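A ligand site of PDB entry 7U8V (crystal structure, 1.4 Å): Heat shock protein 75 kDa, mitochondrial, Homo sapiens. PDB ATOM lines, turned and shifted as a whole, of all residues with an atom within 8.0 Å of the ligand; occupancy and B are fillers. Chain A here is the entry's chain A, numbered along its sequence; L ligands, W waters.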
ATOM      1  N   TYR A 429     -34.056   7.373  -2.162  1.00  0.00           N
ATOM      2  CA  TYR A 429     -32.786   7.455  -2.865  1.00  0.00           C
ATOM      3  C   TYR A 429     -32.965   7.158  -4.337  1.00  0.00           C
ATOM      4  O   TYR A 429     -33.710   6.246  -4.718  1.00  0.00           O
ATOM      5  CB  TYR A 429     -31.766   6.478  -2.253  1.00  0.00           C
ATOM      6  CG  TYR A 429     -31.423   6.846  -0.837  1.00  0.00           C
ATOM      7  CD1 TYR A 429     -30.470   7.819  -0.568  1.00  0.00           C
ATOM      8  CD2 TYR A 429     -32.109   6.270   0.226  1.00  0.00           C
ATOM      9  CE1 TYR A 429     -30.176   8.180   0.737  1.00  0.00           C
ATOM     10  CE2 TYR A 429     -31.808   6.621   1.538  1.00  0.00           C
ATOM     11  CZ  TYR A 429     -30.849   7.582   1.780  1.00  0.00           C
ATOM     12  OH  TYR A 429     -30.569   7.943   3.085  1.00  0.00           O
ATOM     13  N   TYR A 444     -21.299   3.776  -5.953  1.00  0.00           N
ATOM     14  CA  TYR A 444     -22.128   4.198  -4.834  1.00  0.00           C
ATOM     15  C   TYR A 444     -23.286   3.243  -4.624  1.00  0.00           C
ATOM     16  O   TYR A 444     -23.556   2.810  -3.497  1.00  0.00           O
ATOM     17  CB  TYR A 444     -22.637   5.628  -5.061  1.00  0.00           C
ATOM     18  CG  TYR A 444     -21.520   6.642  -5.076  1.00  0.00           C
ATOM     19  CD1 TYR A 444     -21.111   7.259  -3.902  1.00  0.00           C
ATOM     20  CD2 TYR A 444     -20.857   6.960  -6.254  1.00  0.00           C
ATOM     21  CE1 TYR A 444     -20.089   8.172  -3.905  1.00  0.00           C
ATOM     22  CE2 TYR A 444     -19.827   7.883  -6.263  1.00  0.00           C
ATOM     23  CZ  TYR A 444     -19.447   8.484  -5.086  1.00  0.00           C
ATOM     24  OH  TYR A 444     -18.411   9.401  -5.098  1.00  0.00           O
ATOM     25  N   TYR A 445     -23.969   2.871  -5.702  1.00  0.00           N
ATOM     26  CA  TYR A 445     -25.036   1.890  -5.565  1.00  0.00           C
ATOM     27  C   TYR A 445     -24.503   0.544  -5.077  1.00  0.00           C
ATOM     28  O   TYR A 445     -25.106  -0.083  -4.197  1.00  0.00           O
ATOM     29  CB  TYR A 445     -25.826   1.732  -6.860  1.00  0.00           C
ATOM     30  CG  TYR A 445     -26.729   0.564  -6.689  1.00  0.00           C
ATOM     31  CD1 TYR A 445     -27.803   0.641  -5.811  1.00  0.00           C
ATOM     32  CD2 TYR A 445     -26.466  -0.645  -7.326  1.00  0.00           C
ATOM     33  CE1 TYR A 445     -28.611  -0.441  -5.581  1.00  0.00           C
ATOM     34  CE2 TYR A 445     -27.289  -1.735  -7.111  1.00  0.00           C
ATOM     35  CZ  TYR A 445     -28.354  -1.618  -6.238  1.00  0.00           C
ATOM     36  OH  TYR A 445     -29.170  -2.696  -5.997  1.00  0.00           O
ATOM     37  N   ALA A 447     -22.081  -0.156  -3.177  1.00  0.00           N
ATOM     38  CA  ALA A 447     -21.855  -0.123  -1.736  1.00  0.00           C
ATOM     39  C   ALA A 447     -23.172  -0.129  -0.971  1.00  0.00           C
ATOM     40  O   ALA A 447     -23.310  -0.812   0.046  1.00  0.00           O
ATOM     41  CB  ALA A 447     -21.021   1.108  -1.376  1.00  0.00           C
ATOM     42  N   MET A 448     -24.157   0.628  -1.456  1.00  0.00           N
ATOM     43  CA  MET A 448     -25.443   0.694  -0.758  1.00  0.00           C
ATOM     44  C   MET A 448     -26.175  -0.633  -0.756  1.00  0.00           C
ATOM     45  O   MET A 448     -26.950  -0.902   0.159  1.00  0.00           O
ATOM     46  CB  MET A 448     -26.333   1.749  -1.422  1.00  0.00           C
ATOM     47  CG  MET A 448     -25.832   3.166  -1.154  1.00  0.00           C
ATOM     48  SD  MET A 448     -26.850   4.394  -1.988  1.00  0.00           S
ATOM     49  CE  MET A 448     -28.429   4.181  -1.181  1.00  0.00           C
ATOM     50  N   ILE A 479     -32.998  12.022  -2.399  1.00  0.00           N
ATOM     51  CA  ILE A 479     -31.536  12.148  -2.304  1.00  0.00           C
ATOM     52  C   ILE A 479     -30.902  11.418  -3.476  1.00  0.00           C
ATOM     53  O   ILE A 479     -31.113  10.207  -3.635  1.00  0.00           O
ATOM     54  CB  ILE A 479     -31.012  11.582  -0.972  1.00  0.00           C
ATOM     55  CG1 ILE A 479     -31.581  12.363   0.199  1.00  0.00           C
ATOM     56  CG2 ILE A 479     -29.476  11.618  -0.945  1.00  0.00           C
ATOM     57  CD1 ILE A 479     -31.133  11.858   1.555  1.00  0.00           C
ATOM     58  N   SER A 480     -30.119  12.135  -4.274  1.00  0.00           N
ATOM     59  CA  SER A 480     -29.333  11.499  -5.329  1.00  0.00           C
ATOM     60  C   SER A 480     -28.120  10.809  -4.727  1.00  0.00           C
ATOM     61  O   SER A 480     -27.363  11.436  -3.965  1.00  0.00           O
ATOM     62  CB  SER A 480     -28.873  12.515  -6.367  1.00  0.00           C
ATOM     63  OG  SER A 480     -28.002  11.887  -7.300  1.00  0.00           O
ATOM     64  N   VAL A 481     -27.901   9.549  -5.084  1.00  0.00           N
ATOM     65  CA  VAL A 481     -26.810   8.789  -4.469  1.00  0.00           C
ATOM     66  C   VAL A 481     -25.451   9.178  -5.014  1.00  0.00           C
ATOM     67  O   VAL A 481     -24.433   8.782  -4.425  1.00  0.00           O
ATOM     68  CB  VAL A 481     -27.053   7.269  -4.484  1.00  0.00           C
ATOM     69  CG1 VAL A 481     -28.452   6.939  -3.970  1.00  0.00           C
ATOM     70  CG2 VAL A 481     -26.865   6.708  -5.885  1.00  0.00           C
ATOM     71  N   GLU A 482     -25.411   9.914  -6.117  1.00  0.00           N
ATOM     72  CA  GLU A 482     -24.187  10.510  -6.635  1.00  0.00           C
ATOM     73  C   GLU A 482     -24.390  12.009  -6.775  1.00  0.00           C
ATOM     74  O   GLU A 482     -25.435  12.449  -7.281  1.00  0.00           O
ATOM     75  CB  GLU A 482     -23.809   9.922  -8.000  1.00  0.00           C
ATOM     76  CG  GLU A 482     -23.528   8.432  -7.985  1.00  0.00           C
ATOM     77  CD  GLU A 482     -23.077   7.910  -9.333  1.00  0.00           C
ATOM     78  OE1 GLU A 482     -23.387   8.559 -10.359  1.00  0.00           O
ATOM     79  OE2 GLU A 482     -22.406   6.851  -9.375  1.00  0.00           O
ATOM     80  N   THR A 483     -23.422  12.801  -6.342  1.00  0.00           N
ATOM     81  CA  THR A 483     -23.528  14.257  -6.423  1.00  0.00           C
ATOM     82  C   THR A 483     -23.048  14.783  -7.778  1.00  0.00           C
ATOM     83  O   THR A 483     -22.949  16.004  -7.972  1.00  0.00           O
ATOM     84  CB  THR A 483     -22.706  14.950  -5.320  1.00  0.00           C
ATOM     85  OG1 THR A 483     -21.356  14.472  -5.364  1.00  0.00           O
ATOM     86  CG2 THR A 483     -23.311  14.675  -3.952  1.00  0.00           C
HETATM   87  C1  LIG L   1     -19.744  12.895  -2.515  1.00  0.00           C
HETATM   88  C2  LIG L   1     -18.603  12.138  -2.233  1.00  0.00           C
HETATM   89  C3  LIG L   1     -17.428  12.766  -1.864  1.00  0.00           C
HETATM   90  C4  LIG L   1     -17.410  14.135  -1.816  1.00  0.00           C
HETATM   91  C5  LIG L   1     -18.530  14.880  -2.091  1.00  0.00           C
HETATM   92  C6  LIG L   1     -19.711  14.267  -2.476  1.00  0.00           C
HETATM   93  C7  LIG L   1     -20.953  12.094  -2.944  1.00  0.00           C
HETATM   94  C8  LIG L   1     -18.366  16.374  -2.023  1.00  0.00           C
HETATM   95  O1  LIG L   1     -17.811  16.888  -1.116  1.00  0.00           O
HETATM   96  N1  LIG L   1     -18.810  17.198  -3.131  1.00  0.00           N
HETATM   97  O2  LIG L   1     -21.344  12.208  -4.058  1.00  0.00           O
HETATM   98  N2  LIG L   1     -21.517  11.154  -2.028  1.00  0.00           N
HETATM   99  C9  LIG L   1     -21.093  10.966  -0.792  1.00  0.00           C
HETATM  100  C10 LIG L   1     -21.871   9.947  -0.191  1.00  0.00           C
HETATM  101  C11 LIG L   1     -22.775   9.571  -1.145  1.00  0.00           C
HETATM  102  C12 LIG L   1     -22.542  10.341  -2.329  1.00  0.00           C
HETATM  103  C13 LIG L   1     -19.417  16.781  -4.237  1.00  0.00           C
HETATM  104  C14 LIG L   1     -19.668  17.909  -5.057  1.00  0.00           C
HETATM  105  C15 LIG L   1     -19.192  19.003  -4.369  1.00  0.00           C
HETATM  106  C16 LIG L   1     -18.652  18.512  -3.147  1.00  0.00           C
HETATM  107  C17 LIG L   1     -21.865   9.351   1.089  1.00  0.00           C
HETATM  108  C18 LIG L   1     -22.784   8.355   1.383  1.00  0.00           C
HETATM  109  C19 LIG L   1     -23.702   7.960   0.400  1.00  0.00           C
HETATM  110  C20 LIG L   1     -23.709   8.545  -0.852  1.00  0.00           C
HETATM  111  C21 LIG L   1     -20.269  18.077  -6.325  1.00  0.00           C
HETATM  112  C22 LIG L   1     -20.380  19.355  -6.867  1.00  0.00           C
HETATM  113  C23 LIG L   1     -19.898  20.451  -6.167  1.00  0.00           C
HETATM  114  C24 LIG L   1     -19.296  20.294  -4.927  1.00  0.00           C
HETATM  115  O3  LIG L   1     -18.616  10.736  -2.294  1.00  0.00           O
HETATM  116  O   HOH W   1     -19.658  18.803   0.603  1.00  0.00           O
HETATM  117  O   HOH W   2     -20.969  21.314  -2.089  1.00  0.00           O
HETATM  118  O   HOH W   3     -17.114  16.886   1.408  1.00  0.00           O
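O2 of the ligand lies within hydrogen-bond range of N of Thr 483 (3.1 Å).
OG1 of Thr 483 sits at hydrogen-bond distance from O2 of the ligand (2.6 Å).
An oxygen (O3) of the ligand lies within hydrogen-bond range of the side-chain hydroxyl (OH) of Tyr 444, 3.1 Å away.
O of Val 481 touches C12 of the ligand, at 3.2 Å.
Hydrophobic or aromatic side chains within 4 Å of the ligand: Tyr 444.
Of the 10 residues printed, 3 come within 4 Å of the ligand.
The nearest printed residue that does not touch the ligand is Glu 482 (4.1 Å).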
